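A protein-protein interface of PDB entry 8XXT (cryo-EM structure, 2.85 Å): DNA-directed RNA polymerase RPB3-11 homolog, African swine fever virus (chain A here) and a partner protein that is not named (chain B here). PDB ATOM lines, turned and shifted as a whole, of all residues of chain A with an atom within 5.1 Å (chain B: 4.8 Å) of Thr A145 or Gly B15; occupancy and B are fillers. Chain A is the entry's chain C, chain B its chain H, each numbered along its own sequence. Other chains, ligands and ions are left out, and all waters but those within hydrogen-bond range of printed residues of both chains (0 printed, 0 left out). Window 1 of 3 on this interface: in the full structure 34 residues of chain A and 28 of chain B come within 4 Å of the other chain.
Among the printed residues, merely in contact across the chains: Phe A29 with Ala B19 (3.5 Å), Leu A35 with Thr B16 (3.6 Å), Leu A35 with Tyr B17 (3.99 Å), Tyr A125 with Ala B19 (3.9 Å), Asn A143 with Thr B16 (3.2 Å), Thr A145 with Gly B15 (3.6 Å), Phe A146 with Val B5 (3.5 Å), Phe A146 with Gly B15 (3.5 Å), Phe A146 with Thr B16 (3.0 Å) and Glu A147 with Ala B18 (3.97 Å).
N of Ser A126 is in hydrogen-bond range of O of Phe A146 (2.8 Å). The side-chain hydroxyl of Thr B16 is in hydrogen-bond range of the backbone carbonyl oxygen of Pro B13 (3.4 Å). O of Asn A143 sits at hydrogen-bond distance from OG of Ser A126 (2.8 Å). N of Gly B15 lies within hydrogen-bond range of O of Val B5, at 2.7 Å.
The side-chain hydroxyl of Thr A145 is in hydrogen-bond range of the backbone carbonyl oxygen of Thr B16.
Of the 10 printed residues of chain A, 7 touch a printed residue of chain B. Printed residues of chain A that touch a printed residue of chain B: Phe A29, Leu A35, Tyr A125, Asn A143, Thr A145, Phe A146 and Glu A147. Among the printed residues, 11 pairs touch across the chains. Among the printed residues, no Asp or Glu carboxylate lies within 4 Å of a Lys or Arg side-chain nitrogen of the other chain.
Of the printed residues of chain B, Phe A146 touches Val B5, Gly B15 and Thr B16. Of the printed residues of chain B, Glu A147 touches Ala B18 (3.97 Å). Printed residues of chain A within 4 Å of Val B5: Phe A146. Val B6 touches none of the printed residues of chain A. Ile B14 touches none of the printed residues of chain A. Of chain A, only Thr A145 (3.6 Å) and Phe A146 (3.5 Å) come within 4 Å of Gly B15. Of the printed residues of chain A, Thr B16 touches Leu A35 (3.6 Å), Asn A143 (3.2 Å), Thr A145 (2.4 Å) and Phe A146 (3.0 Å). Printed residues of chain A within 4 Å of Ala B19: Phe A29 and Tyr A125. The nearest residue of chain B that does not touch Thr A145 is Ala B19 (4.1 Å).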
ATOM      1  N   PHE A  29     -34.989 -28.778 -25.429  1.00  0.00           N
ATOM      2  CA  PHE A  29     -35.067 -28.934 -26.871  1.00  0.00           C
ATOM      3  C   PHE A  29     -36.317 -29.658 -27.343  1.00  0.00           C
ATOM      4  O   PHE A  29     -36.568 -29.689 -28.553  1.00  0.00           O
ATOM      5  CB  PHE A  29     -33.836 -29.684 -27.397  1.00  0.00           C
ATOM      6  CG  PHE A  29     -32.571 -28.896 -27.306  1.00  0.00           C
ATOM      7  CD1 PHE A  29     -32.469 -27.659 -27.913  1.00  0.00           C
ATOM      8  CD2 PHE A  29     -31.479 -29.395 -26.620  1.00  0.00           C
ATOM      9  CE1 PHE A  29     -31.310 -26.930 -27.827  1.00  0.00           C
ATOM     10  CE2 PHE A  29     -30.316 -28.672 -26.542  1.00  0.00           C
ATOM     11  CZ  PHE A  29     -30.233 -27.435 -27.141  1.00  0.00           C
ATOM     12  N   LEU A  35     -30.457 -37.209 -32.719  1.00  0.00           N
ATOM     13  CA  LEU A  35     -30.327 -35.987 -33.489  1.00  0.00           C
ATOM     14  C   LEU A  35     -30.144 -36.307 -34.971  1.00  0.00           C
ATOM     15  O   LEU A  35     -29.685 -37.395 -35.326  1.00  0.00           O
ATOM     16  CB  LEU A  35     -29.152 -35.168 -32.969  1.00  0.00           C
ATOM     17  CG  LEU A  35     -29.502 -34.361 -31.722  1.00  0.00           C
ATOM     18  CD1 LEU A  35     -28.255 -33.967 -30.964  1.00  0.00           C
ATOM     19  CD2 LEU A  35     -30.306 -33.140 -32.114  1.00  0.00           C
ATOM     20  N   TYR A 125     -29.978 -20.639 -30.026  1.00  0.00           N
ATOM     21  CA  TYR A 125     -29.560 -21.984 -30.382  1.00  0.00           C
ATOM     22  C   TYR A 125     -29.412 -22.098 -31.893  1.00  0.00           C
ATOM     23  O   TYR A 125     -29.843 -21.232 -32.654  1.00  0.00           O
ATOM     24  CB  TYR A 125     -30.552 -23.016 -29.849  1.00  0.00           C
ATOM     25  CG  TYR A 125     -30.577 -23.085 -28.344  1.00  0.00           C
ATOM     26  CD1 TYR A 125     -29.490 -23.577 -27.638  1.00  0.00           C
ATOM     27  CD2 TYR A 125     -31.680 -22.650 -27.628  1.00  0.00           C
ATOM     28  CE1 TYR A 125     -29.504 -23.639 -26.262  1.00  0.00           C
ATOM     29  CE2 TYR A 125     -31.701 -22.708 -26.249  1.00  0.00           C
ATOM     30  CZ  TYR A 125     -30.610 -23.204 -25.573  1.00  0.00           C
ATOM     31  OH  TYR A 125     -30.625 -23.265 -24.201  1.00  0.00           O
ATOM     32  N   SER A 126     -28.779 -23.189 -32.323  1.00  0.00           N
ATOM     33  CA  SER A 126     -28.579 -23.407 -33.748  1.00  0.00           C
ATOM     34  C   SER A 126     -29.895 -23.570 -34.495  1.00  0.00           C
ATOM     35  O   SER A 126     -29.933 -23.363 -35.711  1.00  0.00           O
ATOM     36  CB  SER A 126     -27.696 -24.629 -33.971  1.00  0.00           C
ATOM     37  OG  SER A 126     -27.667 -24.992 -35.334  1.00  0.00           O
ATOM     38  N   ARG A 127     -30.971 -23.933 -33.798  1.00  0.00           N
ATOM     39  CA  ARG A 127     -32.277 -24.024 -34.437  1.00  0.00           C
ATOM     40  C   ARG A 127     -32.804 -22.664 -34.864  1.00  0.00           C
ATOM     41  O   ARG A 127     -33.771 -22.602 -35.629  1.00  0.00           O
ATOM     42  CB  ARG A 127     -33.279 -24.688 -33.497  1.00  0.00           C
ATOM     43  CG  ARG A 127     -33.380 -24.026 -32.141  1.00  0.00           C
ATOM     44  CD  ARG A 127     -34.829 -23.830 -31.732  1.00  0.00           C
ATOM     45  NE  ARG A 127     -34.962 -23.548 -30.309  1.00  0.00           N
ATOM     46  CZ  ARG A 127     -34.877 -24.463 -29.353  1.00  0.00           C
ATOM     47  NH1 ARG A 127     -34.670 -25.738 -29.633  1.00  0.00           N
ATOM     48  NH2 ARG A 127     -35.005 -24.087 -28.083  1.00  0.00           N
ATOM     49  N   ASN A 143     -26.913 -29.759 -36.481  1.00  0.00           N
ATOM     50  CA  ASN A 143     -27.769 -30.067 -35.353  1.00  0.00           C
ATOM     51  C   ASN A 143     -28.388 -28.787 -34.796  1.00  0.00           C
ATOM     52  O   ASN A 143     -27.740 -27.739 -34.760  1.00  0.00           O
ATOM     53  CB  ASN A 143     -26.978 -30.775 -34.261  1.00  0.00           C
ATOM     54  CG  ASN A 143     -26.834 -32.250 -34.521  1.00  0.00           C
ATOM     55  OD1 ASN A 143     -26.506 -33.022 -33.625  1.00  0.00           O
ATOM     56  ND2 ASN A 143     -27.090 -32.655 -35.750  1.00  0.00           N
ATOM     57  N   PRO A 144     -29.643 -28.846 -34.350  1.00  0.00           N
ATOM     58  CA  PRO A 144     -30.299 -27.663 -33.792  1.00  0.00           C
ATOM     59  C   PRO A 144     -30.015 -27.411 -32.320  1.00  0.00           C
ATOM     60  O   PRO A 144     -30.689 -26.574 -31.717  1.00  0.00           O
ATOM     61  CB  PRO A 144     -31.784 -27.985 -34.008  1.00  0.00           C
ATOM     62  CG  PRO A 144     -31.847 -29.459 -33.882  1.00  0.00           C
ATOM     63  CD  PRO A 144     -30.560 -29.994 -34.446  1.00  0.00           C
ATOM     64  N   THR A 145     -29.047 -28.101 -31.725  1.00  0.00           N
ATOM     65  CA  THR A 145     -28.777 -27.987 -30.300  1.00  0.00           C
ATOM     66  C   THR A 145     -27.527 -27.181 -29.983  1.00  0.00           C
ATOM     67  O   THR A 145     -27.138 -27.107 -28.815  1.00  0.00           O
ATOM     68  CB  THR A 145     -28.649 -29.375 -29.675  1.00  0.00           C
ATOM     69  OG1 THR A 145     -27.453 -30.003 -30.149  1.00  0.00           O
ATOM     70  CG2 THR A 145     -29.840 -30.230 -30.041  1.00  0.00           C
ATOM     71  N   PHE A 146     -26.886 -26.584 -30.979  1.00  0.00           N
ATOM     72  CA  PHE A 146     -25.664 -25.836 -30.724  1.00  0.00           C
ATOM     73  C   PHE A 146     -25.983 -24.534 -30.012  1.00  0.00           C
ATOM     74  O   PHE A 146     -26.919 -23.821 -30.385  1.00  0.00           O
ATOM     75  CB  PHE A 146     -24.931 -25.552 -32.027  1.00  0.00           C
ATOM     76  CG  PHE A 146     -24.167 -26.716 -32.547  1.00  0.00           C
ATOM     77  CD1 PHE A 146     -22.961 -27.073 -31.982  1.00  0.00           C
ATOM     78  CD2 PHE A 146     -24.657 -27.462 -33.597  1.00  0.00           C
ATOM     79  CE1 PHE A 146     -22.257 -28.145 -32.459  1.00  0.00           C
ATOM     80  CE2 PHE A 146     -23.957 -28.534 -34.077  1.00  0.00           C
ATOM     81  CZ  PHE A 146     -22.756 -28.876 -33.508  1.00  0.00           C
ATOM     82  N   GLU A 147     -25.198 -24.219 -28.990  1.00  0.00           N
ATOM     83  CA  GLU A 147     -25.364 -22.975 -28.252  1.00  0.00           C
ATOM     84  C   GLU A 147     -24.602 -21.871 -28.970  1.00  0.00           C
ATOM     85  O   GLU A 147     -23.368 -21.852 -28.964  1.00  0.00           O
ATOM     86  CB  GLU A 147     -24.859 -23.129 -26.821  1.00  0.00           C
ATOM     87  CG  GLU A 147     -25.939 -23.133 -25.766  1.00  0.00           C
ATOM     88  CD  GLU A 147     -25.390 -23.466 -24.396  1.00  0.00           C
ATOM     89  OE1 GLU A 147     -24.259 -23.986 -24.321  1.00  0.00           O
ATOM     90  OE2 GLU A 147     -26.088 -23.207 -23.395  1.00  0.00           O
ATOM     91  N   PRO B   4     -17.362 -24.380 -25.689  1.00  0.00           N
ATOM     92  CA  PRO B   4     -17.014 -24.215 -27.101  1.00  0.00           C
ATOM     93  C   PRO B   4     -17.819 -25.149 -27.987  1.00  0.00           C
ATOM     94  O   PRO B   4     -18.211 -26.243 -27.579  1.00  0.00           O
ATOM     95  CB  PRO B   4     -15.521 -24.553 -27.140  1.00  0.00           C
ATOM     96  CG  PRO B   4     -15.271 -25.337 -25.898  1.00  0.00           C
ATOM     97  CD  PRO B   4     -16.199 -24.771 -24.881  1.00  0.00           C
ATOM     98  N   VAL B   5     -18.081 -24.687 -29.210  1.00  0.00           N
ATOM     99  CA  VAL B   5     -18.873 -25.471 -30.151  1.00  0.00           C
ATOM    100  C   VAL B   5     -18.204 -26.810 -30.421  1.00  0.00           C
ATOM    101  O   VAL B   5     -18.871 -27.845 -30.531  1.00  0.00           O
ATOM    102  CB  VAL B   5     -19.097 -24.674 -31.447  1.00  0.00           C
ATOM    103  CG1 VAL B   5     -19.859 -25.504 -32.446  1.00  0.00           C
ATOM    104  CG2 VAL B   5     -19.846 -23.401 -31.150  1.00  0.00           C
ATOM    105  N   VAL B   6     -16.882 -26.814 -30.533  1.00  0.00           N
ATOM    106  CA  VAL B   6     -16.111 -28.037 -30.683  1.00  0.00           C
ATOM    107  C   VAL B   6     -14.996 -28.024 -29.653  1.00  0.00           C
ATOM    108  O   VAL B   6     -14.568 -26.964 -29.190  1.00  0.00           O
ATOM    109  CB  VAL B   6     -15.530 -28.189 -32.102  1.00  0.00           C
ATOM    110  CG1 VAL B   6     -16.642 -28.308 -33.121  1.00  0.00           C
ATOM    111  CG2 VAL B   6     -14.632 -27.017 -32.422  1.00  0.00           C
ATOM    112  N   PRO B  13     -17.383 -32.195 -31.813  1.00  0.00           N
ATOM    113  CA  PRO B  13     -18.442 -31.224 -31.515  1.00  0.00           C
ATOM    114  C   PRO B  13     -19.133 -31.464 -30.183  1.00  0.00           C
ATOM    115  O   PRO B  13     -20.236 -32.012 -30.141  1.00  0.00           O
ATOM    116  CB  PRO B  13     -19.413 -31.407 -32.686  1.00  0.00           C
ATOM    117  CG  PRO B  13     -19.208 -32.807 -33.113  1.00  0.00           C
ATOM    118  CD  PRO B  13     -17.749 -33.082 -32.929  1.00  0.00           C
ATOM    119  N   ILE B  14     -18.496 -31.047 -29.087  1.00  0.00           N
ATOM    120  CA  ILE B  14     -19.136 -31.123 -27.779  1.00  0.00           C
ATOM    121  C   ILE B  14     -20.228 -30.073 -27.632  1.00  0.00           C
ATOM    122  O   ILE B  14     -21.101 -30.200 -26.763  1.00  0.00           O
ATOM    123  CB  ILE B  14     -18.088 -30.981 -26.662  1.00  0.00           C
ATOM    124  CG1 ILE B  14     -17.427 -29.606 -26.724  1.00  0.00           C
ATOM    125  CG2 ILE B  14     -17.045 -32.070 -26.774  1.00  0.00           C
ATOM    126  CD1 ILE B  14     -16.337 -29.414 -25.709  1.00  0.00           C
ATOM    127  N   GLY B  15     -20.207 -29.034 -28.467  1.00  0.00           N
ATOM    128  CA  GLY B  15     -21.250 -28.030 -28.421  1.00  0.00           C
ATOM    129  C   GLY B  15     -22.617 -28.562 -28.781  1.00  0.00           C
ATOM    130  O   GLY B  15     -23.623 -27.930 -28.450  1.00  0.00           O
ATOM    131  N   THR B  16     -22.677 -29.709 -29.461  1.00  0.00           N
ATOM    132  CA  THR B  16     -23.963 -30.329 -29.757  1.00  0.00           C
ATOM    133  C   THR B  16     -24.702 -30.670 -28.473  1.00  0.00           C
ATOM    134  O   THR B  16     -25.894 -30.385 -28.329  1.00  0.00           O
ATOM    135  CB  THR B  16     -23.762 -31.594 -30.586  1.00  0.00           C
ATOM    136  OG1 THR B  16     -23.101 -31.274 -31.813  1.00  0.00           O
ATOM    137  CG2 THR B  16     -25.093 -32.223 -30.899  1.00  0.00           C
ATOM    138  N   TYR B  17     -24.000 -31.282 -27.529  1.00  0.00           N
ATOM    139  CA  TYR B  17     -24.585 -31.727 -26.279  1.00  0.00           C
ATOM    140  C   TYR B  17     -24.280 -30.795 -25.123  1.00  0.00           C
ATOM    141  O   TYR B  17     -24.586 -31.139 -23.983  1.00  0.00           O
ATOM    142  CB  TYR B  17     -24.085 -33.132 -25.945  1.00  0.00           C
ATOM    143  CG  TYR B  17     -23.980 -34.039 -27.145  1.00  0.00           C
ATOM    144  CD1 TYR B  17     -25.099 -34.359 -27.897  1.00  0.00           C
ATOM    145  CD2 TYR B  17     -22.756 -34.563 -27.534  1.00  0.00           C
ATOM    146  CE1 TYR B  17     -25.004 -35.185 -28.999  1.00  0.00           C
ATOM    147  CE2 TYR B  17     -22.650 -35.389 -28.633  1.00  0.00           C
ATOM    148  CZ  TYR B  17     -23.776 -35.697 -29.362  1.00  0.00           C
ATOM    149  OH  TYR B  17     -23.677 -36.521 -30.457  1.00  0.00           O
ATOM    150  N   ALA B  18     -23.665 -29.639 -25.380  1.00  0.00           N
ATOM    151  CA  ALA B  18     -23.337 -28.717 -24.295  1.00  0.00           C
ATOM    152  C   ALA B  18     -24.589 -28.234 -23.570  1.00  0.00           C
ATOM    153  O   ALA B  18     -24.628 -28.190 -22.333  1.00  0.00           O
ATOM    154  CB  ALA B  18     -22.552 -27.530 -24.845  1.00  0.00           C
ATOM    155  N   ALA B  19     -25.621 -27.853 -24.326  1.00  0.00           N
ATOM    156  CA  ALA B  19     -26.831 -27.322 -23.706  1.00  0.00           C
ATOM    157  C   ALA B  19     -27.538 -28.377 -22.866  1.00  0.00           C
ATOM    158  O   ALA B  19     -28.018 -28.085 -21.766  1.00  0.00           O
ATOM    159  CB  ALA B  19     -27.766 -26.770 -24.779  1.00  0.00           C
